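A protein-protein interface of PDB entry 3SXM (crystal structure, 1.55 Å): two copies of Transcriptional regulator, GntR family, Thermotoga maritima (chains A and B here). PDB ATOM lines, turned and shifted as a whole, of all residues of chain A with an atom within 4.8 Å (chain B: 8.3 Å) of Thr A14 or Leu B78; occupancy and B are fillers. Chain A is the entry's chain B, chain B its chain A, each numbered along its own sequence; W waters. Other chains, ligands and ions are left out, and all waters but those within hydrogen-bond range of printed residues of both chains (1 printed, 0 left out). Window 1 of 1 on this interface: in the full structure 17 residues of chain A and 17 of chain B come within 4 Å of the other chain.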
ATOM      1  N   GLU A  10      12.549   3.085  -5.812  1.00  0.00           N
ATOM      2  CA  GLU A  10      11.766   4.290  -5.545  1.00  0.00           C
ATOM      3  C   GLU A  10      10.945   4.690  -6.748  1.00  0.00           C
ATOM      4  O   GLU A  10       9.812   5.173  -6.612  1.00  0.00           O
ATOM      5  CB  GLU A  10      12.616   5.462  -5.096  1.00  0.00           C
ATOM      6  CG  GLU A  10      13.246   5.362  -3.734  1.00  0.00           C
ATOM      7  CD  GLU A  10      14.052   6.628  -3.414  1.00  0.00           C
ATOM      8  OE1 GLU A  10      14.313   7.410  -4.353  1.00  0.00           O
ATOM      9  OE2 GLU A  10      14.495   6.750  -2.274  1.00  0.00           O
ATOM     10  N   THR A  11      11.512   4.560  -7.926  1.00  0.00           N
ATOM     11  CA  THR A  11      10.830   4.926  -9.156  1.00  0.00           C
ATOM     12  C   THR A  11       9.603   4.035  -9.338  1.00  0.00           C
ATOM     13  O   THR A  11       8.503   4.526  -9.631  1.00  0.00           O
ATOM     14  CB  THR A  11      11.802   4.747 -10.359  1.00  0.00           C
ATOM     15  OG1 THR A  11      12.972   5.552 -10.215  1.00  0.00           O
ATOM     16  CG2 THR A  11      11.125   5.227 -11.651  1.00  0.00           C
ATOM     17  N   ILE A  12       9.767   2.737  -9.241  1.00  0.00           N
ATOM     18  CA  ILE A  12       8.678   1.801  -9.474  1.00  0.00           C
ATOM     19  C   ILE A  12       7.605   2.007  -8.402  1.00  0.00           C
ATOM     20  O   ILE A  12       6.425   2.002  -8.703  1.00  0.00           O
ATOM     21  CB  ILE A  12       9.199   0.388  -9.470  1.00  0.00           C
ATOM     22  CG1 ILE A  12      10.144   0.133 -10.656  1.00  0.00           C
ATOM     23  CG2 ILE A  12       8.033  -0.609  -9.375  1.00  0.00           C
ATOM     24  CD1 ILE A  12       9.465   0.088 -12.002  1.00  0.00           C
ATOM     25  N   GLU A  13       7.991   2.219  -7.145  1.00  0.00           N
ATOM     26  CA  GLU A  13       6.988   2.432  -6.083  1.00  0.00           C
ATOM     27  C   GLU A  13       6.145   3.662  -6.395  1.00  0.00           C
ATOM     28  O   GLU A  13       4.926   3.678  -6.147  1.00  0.00           O
ATOM     29  CB  GLU A  13       7.636   2.573  -4.725  1.00  0.00           C
ATOM     30  CG  GLU A  13       6.627   2.744  -3.605  1.00  0.00           C
ATOM     31  CD  GLU A  13       7.221   2.774  -2.199  1.00  0.00           C
ATOM     32  OE1 GLU A  13       8.300   3.338  -1.984  1.00  0.00           O
ATOM     33  OE2 GLU A  13       6.589   2.166  -1.298  1.00  0.00           O
ATOM     34  N   THR A  14       6.804   4.706  -6.846  1.00  0.00           N
ATOM     35  CA  THR A  14       6.101   5.955  -7.195  1.00  0.00           C
ATOM     36  C   THR A  14       5.134   5.697  -8.328  1.00  0.00           C
ATOM     37  O   THR A  14       3.992   6.191  -8.312  1.00  0.00           O
ATOM     38  CB  THR A  14       7.098   7.098  -7.519  1.00  0.00           C
ATOM     39  OG1 THR A  14       7.970   7.285  -6.405  1.00  0.00           O
ATOM     40  CG2 THR A  14       6.385   8.408  -7.856  1.00  0.00           C
ATOM     41  N   ARG A  15       5.535   4.917  -9.332  1.00  0.00           N
ATOM     42  CA  ARG A  15       4.630   4.534 -10.388  1.00  0.00           C
ATOM     43  C   ARG A  15       3.438   3.752  -9.886  1.00  0.00           C
ATOM     44  O   ARG A  15       2.308   3.983 -10.337  1.00  0.00           O
ATOM     45  CB  ARG A  15       5.357   3.729 -11.456  1.00  0.00           C
ATOM     46  CG  ARG A  15       6.380   4.517 -12.239  1.00  0.00           C
ATOM     47  CD  ARG A  15       6.995   3.700 -13.388  1.00  0.00           C
ATOM     48  NE  ARG A  15       6.031   3.416 -14.393  1.00  0.00           N
ATOM     49  CZ  ARG A  15       6.207   2.604 -15.440  1.00  0.00           C
ATOM     50  NH1 ARG A  15       7.426   2.097 -15.714  1.00  0.00           N
ATOM     51  NH2 ARG A  15       5.191   2.339 -16.246  1.00  0.00           N
ATOM     52  N   ILE A  16       3.645   2.814  -8.970  1.00  0.00           N
ATOM     53  CA  ILE A  16       2.542   2.010  -8.430  1.00  0.00           C
ATOM     54  C   ILE A  16       1.578   2.979  -7.735  1.00  0.00           C
ATOM     55  O   ILE A  16       0.388   2.949  -7.976  1.00  0.00           O
ATOM     56  CB  ILE A  16       3.037   0.923  -7.481  1.00  0.00           C
ATOM     57  CG1 ILE A  16       3.830  -0.187  -8.264  1.00  0.00           C
ATOM     58  CG2 ILE A  16       1.885   0.320  -6.710  1.00  0.00           C
ATOM     59  CD1 ILE A  16       4.615  -1.102  -7.393  1.00  0.00           C
ATOM     60  N   MET A  17       2.119   3.849  -6.877  1.00  0.00           N
ATOM     61  CA  MET A  17       1.274   4.834  -6.167  1.00  0.00           C
ATOM     62  C   MET A  17       0.363   5.610  -7.129  1.00  0.00           C
ATOM     63  O   MET A  17      -0.858   5.747  -6.887  1.00  0.00           O
ATOM     64  CB  MET A  17       2.162   5.777  -5.350  1.00  0.00           C
ATOM     65  CG  MET A  17       1.390   6.921  -4.681  1.00  0.00           C
ATOM     66  SD  MET A  17       2.458   8.082  -3.842  1.00  0.00           S
ATOM     67  CE  MET A  17       3.265   8.869  -5.249  1.00  0.00           C
ATOM     68  N   MET A  18       0.939   6.157  -8.191  1.00  0.00           N
ATOM     69  CA  MET A  18       0.191   7.073  -9.036  1.00  0.00           C
ATOM     70  C   MET A  18      -0.674   6.290 -10.018  1.00  0.00           C
ATOM     71  O   MET A  18      -1.831   6.595 -10.237  1.00  0.00           O
ATOM     72  CB  MET A  18       1.152   7.992  -9.779  1.00  0.00           C
ATOM     73  CG  MET A  18       1.959   8.880  -8.890  1.00  0.00           C
ATOM     74  SD  MET A  18       3.078  10.032  -9.756  1.00  0.00           S
ATOM     75  CE  MET A  18       1.929  11.113 -10.379  1.00  0.00           C
ATOM     76  N   LEU A  78       2.824  16.002 -12.252  1.00  0.00           N
ATOM     77  CA  LEU A  78       3.809  15.329 -11.411  1.00  0.00           C
ATOM     78  C   LEU A  78       4.328  14.129 -12.191  1.00  0.00           C
ATOM     79  O   LEU A  78       5.509  13.841 -12.121  1.00  0.00           O
ATOM     80  CB  LEU A  78       3.202  14.880 -10.073  1.00  0.00           C
ATOM     81  CG  LEU A  78       2.839  16.039  -9.137  1.00  0.00           C
ATOM     82  CD1 LEU A  78       2.102  15.499  -7.997  1.00  0.00           C
ATOM     83  CD2 LEU A  78       4.069  16.784  -8.692  1.00  0.00           C
ATOM     84  N   ILE A  82       8.326  13.401 -13.492  1.00  0.00           N
ATOM     85  CA  ILE A  82       9.135  12.207 -13.203  1.00  0.00           C
ATOM     86  C   ILE A  82       9.350  11.337 -14.444  1.00  0.00           C
ATOM     87  O   ILE A  82       9.985  10.307 -14.352  1.00  0.00           O
ATOM     88  CB  ILE A  82       8.608  11.366 -12.042  1.00  0.00           C
ATOM     89  CG1 ILE A  82       7.247  10.736 -12.346  1.00  0.00           C
ATOM     90  CG2 ILE A  82       8.593  12.230 -10.761  1.00  0.00           C
ATOM     91  CD1 ILE A  82       6.750   9.702 -11.301  1.00  0.00           C
ATOM     92  N   THR B  14      -4.752  14.772  -4.940  1.00  0.00           N
ATOM     93  CA  THR B  14      -3.321  14.436  -4.918  1.00  0.00           C
ATOM     94  C   THR B  14      -2.868  14.061  -3.530  1.00  0.00           C
ATOM     95  O   THR B  14      -2.099  13.090  -3.340  1.00  0.00           O
ATOM     96  CB  THR B  14      -2.477  15.583  -5.516  1.00  0.00           C
ATOM     97  OG1 THR B  14      -2.930  15.822  -6.845  1.00  0.00           O
ATOM     98  CG2 THR B  14      -1.015  15.250  -5.527  1.00  0.00           C
ATOM     99  N   MET B  17      -4.174  10.501  -2.789  1.00  0.00           N
ATOM    100  CA  MET B  17      -3.278   9.564  -3.507  1.00  0.00           C
ATOM    101  C   MET B  17      -2.005   9.280  -2.712  1.00  0.00           C
ATOM    102  O   MET B  17      -1.645   8.089  -2.523  1.00  0.00           O
ATOM    103  CB  MET B  17      -2.986  10.085  -4.921  1.00  0.00           C
ATOM    104  CG  MET B  17      -1.986   9.219  -5.712  1.00  0.00           C
ATOM    105  SD  MET B  17      -1.609   9.918  -7.300  1.00  0.00           S
ATOM    106  CE  MET B  17      -0.650  11.338  -6.812  1.00  0.00           C
ATOM    107  N   MET B  18      -1.273  10.318  -2.348  1.00  0.00           N
ATOM    108  CA  MET B  18       0.052  10.146  -1.768  1.00  0.00           C
ATOM    109  C   MET B  18      -0.047   9.733  -0.297  1.00  0.00           C
ATOM    110  O   MET B  18       0.638   8.815   0.157  1.00  0.00           O
ATOM    111  CB  MET B  18       0.877  11.417  -1.910  1.00  0.00           C
ATOM    112  CG  MET B  18       1.103  11.838  -3.361  1.00  0.00           C
ATOM    113  SD  MET B  18       2.073  13.319  -3.566  1.00  0.00           S
ATOM    114  CE  MET B  18       3.620  12.724  -3.164  1.00  0.00           C
ATOM    115  N   PHE B  21      -1.592   6.197   0.268  1.00  0.00           N
ATOM    116  CA  PHE B  21      -0.636   5.181  -0.143  1.00  0.00           C
ATOM    117  C   PHE B  21       0.394   4.973   0.957  1.00  0.00           C
ATOM    118  O   PHE B  21       0.754   3.834   1.256  1.00  0.00           O
ATOM    119  CB  PHE B  21       0.088   5.585  -1.450  1.00  0.00           C
ATOM    120  CG  PHE B  21       1.088   4.557  -1.926  1.00  0.00           C
ATOM    121  CD1 PHE B  21       0.679   3.508  -2.714  1.00  0.00           C
ATOM    122  CD2 PHE B  21       2.437   4.649  -1.621  1.00  0.00           C
ATOM    123  CE1 PHE B  21       1.578   2.585  -3.220  1.00  0.00           C
ATOM    124  CE2 PHE B  21       3.314   3.676  -2.051  1.00  0.00           C
ATOM    125  CZ  PHE B  21       2.891   2.672  -2.848  1.00  0.00           C
ATOM    126  N   ILE B  67       4.171  10.650   4.849  1.00  0.00           N
ATOM    127  CA  ILE B  67       4.973  10.615   3.593  1.00  0.00           C
ATOM    128  C   ILE B  67       6.408  10.184   3.913  1.00  0.00           C
ATOM    129  O   ILE B  67       6.997   9.295   3.225  1.00  0.00           O
ATOM    130  CB  ILE B  67       4.952  11.972   2.927  1.00  0.00           C
ATOM    131  CG1 ILE B  67       3.530  12.351   2.505  1.00  0.00           C
ATOM    132  CG2 ILE B  67       5.951  12.067   1.754  1.00  0.00           C
ATOM    133  CD1 ILE B  67       2.944  11.563   1.340  1.00  0.00           C
ATOM    134  N   SER B  70       7.619   6.459   4.373  1.00  0.00           N
ATOM    135  CA  SER B  70       7.910   5.618   3.173  1.00  0.00           C
ATOM    136  C   SER B  70       9.391   5.407   2.998  1.00  0.00           C
ATOM    137  O   SER B  70       9.826   4.408   2.405  1.00  0.00           O
ATOM    138  CB  SER B  70       7.305   6.217   1.892  1.00  0.00           C
ATOM    139  OG  SER B  70       7.993   7.383   1.538  1.00  0.00           O
ATOM    140  N   ASN B  72      10.938   6.847   0.828  1.00  0.00           N
ATOM    141  CA  ASN B  72      11.063   6.964  -0.609  1.00  0.00           C
ATOM    142  C   ASN B  72      11.373   8.428  -0.904  1.00  0.00           C
ATOM    143  O   ASN B  72      10.479   9.268  -0.813  1.00  0.00           O
ATOM    144  CB  ASN B  72       9.781   6.497  -1.295  1.00  0.00           C
ATOM    145  CG  ASN B  72       9.851   6.557  -2.804  1.00  0.00           C
ATOM    146  OD1 ASN B  72      10.423   7.496  -3.378  1.00  0.00           O
ATOM    147  ND2 ASN B  72       9.325   5.548  -3.467  1.00  0.00           N
ATOM    148  N   GLU B  73      12.639   8.710  -1.235  1.00  0.00           N
ATOM    149  CA  GLU B  73      13.036  10.090  -1.412  1.00  0.00           C
ATOM    150  C   GLU B  73      12.304  10.766  -2.577  1.00  0.00           C
ATOM    151  O   GLU B  73      12.103  11.976  -2.580  1.00  0.00           O
ATOM    152  CB  GLU B  73      14.547  10.270  -1.503  1.00  0.00           C
ATOM    153  CG  GLU B  73      15.321   9.807  -0.244  1.00  0.00           C
ATOM    154  CD  GLU B  73      14.947  10.597   1.026  1.00  0.00           C
ATOM    155  OE1 GLU B  73      14.509  11.767   0.938  1.00  0.00           O
ATOM    156  OE2 GLU B  73      15.086  10.036   2.145  1.00  0.00           O
ATOM    157  N   LEU B  74      11.923  10.015  -3.592  1.00  0.00           N
ATOM    158  CA  LEU B  74      11.139  10.586  -4.676  1.00  0.00           C
ATOM    159  C   LEU B  74       9.764  11.007  -4.241  1.00  0.00           C
ATOM    160  O   LEU B  74       9.368  12.133  -4.537  1.00  0.00           O
ATOM    161  CB  LEU B  74      11.118   9.633  -5.918  1.00  0.00           C
ATOM    162  CG  LEU B  74      10.323  10.126  -7.120  1.00  0.00           C
ATOM    163  CD1 LEU B  74      10.860  11.466  -7.569  1.00  0.00           C
ATOM    164  CD2 LEU B  74      10.349   9.139  -8.292  1.00  0.00           C
ATOM    165  N   ILE B  75       9.065  10.165  -3.507  1.00  0.00           N
ATOM    166  CA  ILE B  75       7.737  10.513  -2.968  1.00  0.00           C
ATOM    167  C   ILE B  75       7.853  11.702  -2.046  1.00  0.00           C
ATOM    168  O   ILE B  75       7.063  12.649  -2.153  1.00  0.00           O
ATOM    169  CB  ILE B  75       7.057   9.314  -2.298  1.00  0.00           C
ATOM    170  CG1 ILE B  75       6.756   8.253  -3.334  1.00  0.00           C
ATOM    171  CG2 ILE B  75       5.769   9.779  -1.634  1.00  0.00           C
ATOM    172  CD1 ILE B  75       6.164   6.947  -2.760  1.00  0.00           C
ATOM    173  N   ILE B  76       8.841  11.690  -1.169  1.00  0.00           N
ATOM    174  CA  ILE B  76       9.118  12.790  -0.233  1.00  0.00           C
ATOM    175  C   ILE B  76       9.343  14.068  -1.006  1.00  0.00           C
ATOM    176  O   ILE B  76       8.791  15.123  -0.653  1.00  0.00           O
ATOM    177  CB  ILE B  76      10.266  12.455   0.709  1.00  0.00           C
ATOM    178  CG1 ILE B  76       9.875  11.288   1.647  1.00  0.00           C
ATOM    179  CG2 ILE B  76      10.700  13.662   1.520  1.00  0.00           C
ATOM    180  CD1 ILE B  76      11.033  10.607   2.344  1.00  0.00           C
ATOM    181  N   SER B  77      10.146  14.014  -2.068  1.00  0.00           N
ATOM    182  CA  SER B  77      10.480  15.202  -2.829  1.00  0.00           C
ATOM    183  C   SER B  77       9.267  15.714  -3.596  1.00  0.00           C
ATOM    184  O   SER B  77       9.094  16.950  -3.710  1.00  0.00           O
ATOM    185  CB  SER B  77      11.672  14.919  -3.778  1.00  0.00           C
ATOM    186  OG  SER B  77      11.314  14.192  -4.915  1.00  0.00           O
ATOM    187  N   LEU B  78       8.389  14.843  -4.077  1.00  0.00           N
ATOM    188  CA  LEU B  78       7.194  15.292  -4.806  1.00  0.00           C
ATOM    189  C   LEU B  78       6.248  15.961  -3.836  1.00  0.00           C
ATOM    190  O   LEU B  78       5.634  16.990  -4.168  1.00  0.00           O
ATOM    191  CB  LEU B  78       6.505  14.101  -5.508  1.00  0.00           C
ATOM    192  CG  LEU B  78       7.319  13.485  -6.648  1.00  0.00           C
ATOM    193  CD1 LEU B  78       6.603  12.261  -7.105  1.00  0.00           C
ATOM    194  CD2 LEU B  78       7.465  14.441  -7.802  1.00  0.00           C
ATOM    195  N   TYR B  79       6.162  15.443  -2.625  1.00  0.00           N
ATOM    196  CA  TYR B  79       5.244  16.043  -1.622  1.00  0.00           C
ATOM    197  C   TYR B  79       5.799  17.410  -1.230  1.00  0.00           C
ATOM    198  O   TYR B  79       5.028  18.406  -1.075  1.00  0.00           O
ATOM    199  CB  TYR B  79       5.098  15.158  -0.406  1.00  0.00           C
ATOM    200  CG  TYR B  79       3.921  15.493   0.481  1.00  0.00           C
ATOM    201  CD1 TYR B  79       2.652  15.087   0.153  1.00  0.00           C
ATOM    202  CD2 TYR B  79       4.125  16.174   1.649  1.00  0.00           C
ATOM    203  CE1 TYR B  79       1.556  15.353   1.008  1.00  0.00           C
ATOM    204  CE2 TYR B  79       3.032  16.472   2.494  1.00  0.00           C
ATOM    205  CZ  TYR B  79       1.799  16.068   2.151  1.00  0.00           C
ATOM    206  OH  TYR B  79       0.749  16.376   3.004  1.00  0.00           O
ATOM    207  N   GLU B  80       7.120  17.521  -1.078  1.00  0.00           N
ATOM    208  CA  GLU B  80       7.737  18.808  -0.781  1.00  0.00           C
ATOM    209  C   GLU B  80       7.454  19.803  -1.891  1.00  0.00           C
ATOM    210  O   GLU B  80       7.188  21.011  -1.650  1.00  0.00           O
ATOM    211  CB  GLU B  80       9.220  18.589  -0.639  1.00  0.00           C
ATOM    212  CG  GLU B  80       9.625  18.106   0.692  1.00  0.00           C
ATOM    213  CD  GLU B  80       9.977  19.245   1.622  1.00  0.00           C
ATOM    214  OE1 GLU B  80       9.127  20.132   1.798  1.00  0.00           O
ATOM    215  OE2 GLU B  80      11.111  19.268   2.153  1.00  0.00           O
ATOM    216  N   LYS B  81       7.530  19.337  -3.143  1.00  0.00           N
ATOM    217  CA  LYS B  81       7.275  20.217  -4.273  1.00  0.00           C
ATOM    218  C   LYS B  81       5.881  20.822  -4.276  1.00  0.00           C
ATOM    219  O   LYS B  81       5.742  22.009  -4.665  1.00  0.00           O
ATOM    220  CB  LYS B  81       7.493  19.457  -5.597  1.00  0.00           C
ATOM    221  CG  LYS B  81       7.236  20.276  -6.856  1.00  0.00           C
ATOM    222  CD  LYS B  81       8.362  21.255  -7.144  1.00  0.00           C
ATOM    223  CE  LYS B  81       8.129  22.012  -8.460  1.00  0.00           C
ATOM    224  NZ  LYS B  81       8.642  21.241  -9.631  1.00  0.00           N
ATOM    225  N   ILE B  82       4.905  20.035  -3.844  1.00  0.00           N
ATOM    226  CA  ILE B  82       3.521  20.470  -3.825  1.00  0.00           C
ATOM    227  C   ILE B  82       3.124  21.112  -2.506  1.00  0.00           C
ATOM    228  O   ILE B  82       1.996  21.537  -2.370  1.00  0.00           O
ATOM    229  CB  ILE B  82       2.527  19.416  -4.229  1.00  0.00           C
ATOM    230  CG1 ILE B  82       2.473  18.262  -3.228  1.00  0.00           C
ATOM    231  CG2 ILE B  82       2.823  18.965  -5.668  1.00  0.00           C
ATOM    232  CD1 ILE B  82       1.333  17.245  -3.483  1.00  0.00           C
ATOM    233  N   TRP B  83       4.014  21.168  -1.529  1.00  0.00           N
ATOM    234  CA  TRP B  83       3.650  21.639  -0.204  1.00  0.00           C
ATOM    235  C   TRP B  83       3.125  23.060  -0.206  1.00  0.00           C
ATOM    236  O   TRP B  83       2.114  23.277   0.471  1.00  0.00           O
ATOM    237  CB  TRP B  83       4.802  21.484   0.851  1.00  0.00           C
ATOM    238  CG  TRP B  83       4.318  22.044   2.125  1.00  0.00           C
ATOM    239  CD1 TRP B  83       4.625  23.254   2.616  1.00  0.00           C
ATOM    240  CD2 TRP B  83       3.326  21.480   2.987  1.00  0.00           C
ATOM    241  NE1 TRP B  83       3.907  23.503   3.753  1.00  0.00           N
ATOM    242  CE2 TRP B  83       3.079  22.438   3.990  1.00  0.00           C
ATOM    243  CE3 TRP B  83       2.596  20.280   2.981  1.00  0.00           C
ATOM    244  CZ2 TRP B  83       2.152  22.211   5.025  1.00  0.00           C
ATOM    245  CZ3 TRP B  83       1.698  20.043   4.013  1.00  0.00           C
ATOM    246  CH2 TRP B  83       1.469  21.028   5.009  1.00  0.00           C
ATOM    247  N   ASP B  84       3.725  23.966  -0.934  1.00  0.00           N
ATOM    248  CA  ASP B  84       3.231  25.360  -0.928  1.00  0.00           C
ATOM    249  C   ASP B  84       1.824  25.399  -1.444  1.00  0.00           C
ATOM    250  O   ASP B  84       0.997  26.193  -0.947  1.00  0.00           O
ATOM    251  CB  ASP B  84       4.150  26.277  -1.691  1.00  0.00           C
ATOM    252  CG  ASP B  84       5.378  26.667  -0.903  1.00  0.00           C
ATOM    253  OD1 ASP B  84       5.405  26.431   0.325  1.00  0.00           O
ATOM    254  OD2 ASP B  84       6.338  27.184  -1.528  1.00  0.00           O
ATOM    255  N   ILE B  86      -0.429  22.827  -1.250  1.00  0.00           N
ATOM    256  CA  ILE B  86      -1.172  22.236  -0.152  1.00  0.00           C
ATOM    257  C   ILE B  86      -1.455  23.309   0.919  1.00  0.00           C
ATOM    258  O   ILE B  86      -2.589  23.408   1.428  1.00  0.00           O
ATOM    259  CB  ILE B  86      -0.424  21.030   0.470  1.00  0.00           C
ATOM    260  CG1 ILE B  86      -0.384  19.870  -0.529  1.00  0.00           C
ATOM    261  CG2 ILE B  86      -1.036  20.654   1.802  1.00  0.00           C
ATOM    262  CD1 ILE B  86       0.389  18.663  -0.072  1.00  0.00           C
HETATM  263  O   HOH W   1      10.435   3.076  -0.178  1.00  0.00           O
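ND2 of Asn B72 is in hydrogen-bond range of O of Glu A10, at 3.2 Å.
OE1 of Glu A13 lies within hydrogen-bond range of ND2 of Asn B72, at 2.9 Å.
The side-chain carboxylate (OE2) of Glu A10 is in hydrogen-bond range of the backbone NH (N) of Glu B73.
Water W1 lies within hydrogen-bond range of the side-chain carboxylate (OE1) of Glu A13 (2.8 Å) and the backbone carbonyl oxygen (O) of Ser B70 (3.0 Å).
Printed residues of chain A that touch a printed residue of chain B: Glu A10, Glu A13, Thr A14, Met A17, Met A18, Leu A78 and Ile A82.
Hydrophobic or aromatic side chains of chain A within 4 Å of the printed part of chain B: Met A17, Leu A78 and Ile A82.
Of the 20 printed residues of chain B, 10 touch a printed residue of chain A.
Hydrophobic or aromatic side chains of chain B that line the printed part of chain A: Met B17, Phe B21, Leu B74, Ile B75, Leu B78 and Ile B82.
Among the printed residues, no Asp or Glu carboxylate lies within 4 Å of a Lys or Arg side-chain nitrogen of the other chain.
Thr A14 touches Leu B78, and with the chains exchanged Leu A78 touches Thr B14.
Met B17 touches its own counterpart, Met A17.
Met A17 touches Met B18, and with the chains exchanged Met A18 touches Met B17.
Leu A78 touches Ile B82, and with the chains exchanged Ile A82 touches Leu B78.
N of Asn B72 lies close to OG of Ser B70 (3.1 Å).
OD1 of Asn B72 sits at hydrogen-bond distance from N of Leu B74, at 2.9 Å.
OD1 of Asn B72 lies within hydrogen-bond range of N of Ile B75, 3.0 Å away.
O of Glu B73 lies close to OG of Ser B77 (3.3 Å).
The side-chain hydroxyl (OG) of Ser B77 sits at hydrogen-bond distance from the backbone carbonyl oxygen (O) of Leu B74 (2.9 Å).
O of Glu A10 sits at hydrogen-bond distance from OG1 of Thr A14 (2.8 Å).
Thr A11 touches none of the printed residues of chain B.
Of chain B, only Asn B72, Leu B74, Ile B75 and Leu B78 come within 4 Å of Thr A14.
Arg A15 touches none of the printed residues of chain B.
Printed residues of chain A within 4 Å of Thr B14: Leu A78.
Of the printed residues of chain A, Leu B74 touches Glu A10 (3.6 Å), Thr A14 (3.6 Å) and Ile A82 (3.99 Å).
Leu B78 touches just these residues of chain A: Thr A14 (3.9 Å) and Ile A82 (3.9 Å).
The nearest residue of chain B that does not touch Thr A14 is Phe B21 (6.0 Å).
Leu B74 touches Glu A10.
CE2 of Phe B21 touches OE2 of Glu A13 (3.7 Å).
CD2 of Leu B74 touches OG1 of Thr A14, at 3.6 Å.
CG1 of Ile B75 touches OG1 of Thr A14 (3.4 Å).
CG2 of Thr A14 touches CD1 of Leu B78, at 3.9 Å.
Met B18 touches Met A17 (CA to SD, 3.8 Å).
Met A17 touches Phe B21.
Met A18 touches Met B17.
Thr B14 touches Leu A78.
CD2 of Leu B78 touches CG2 of Ile A82, at 3.9 Å.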
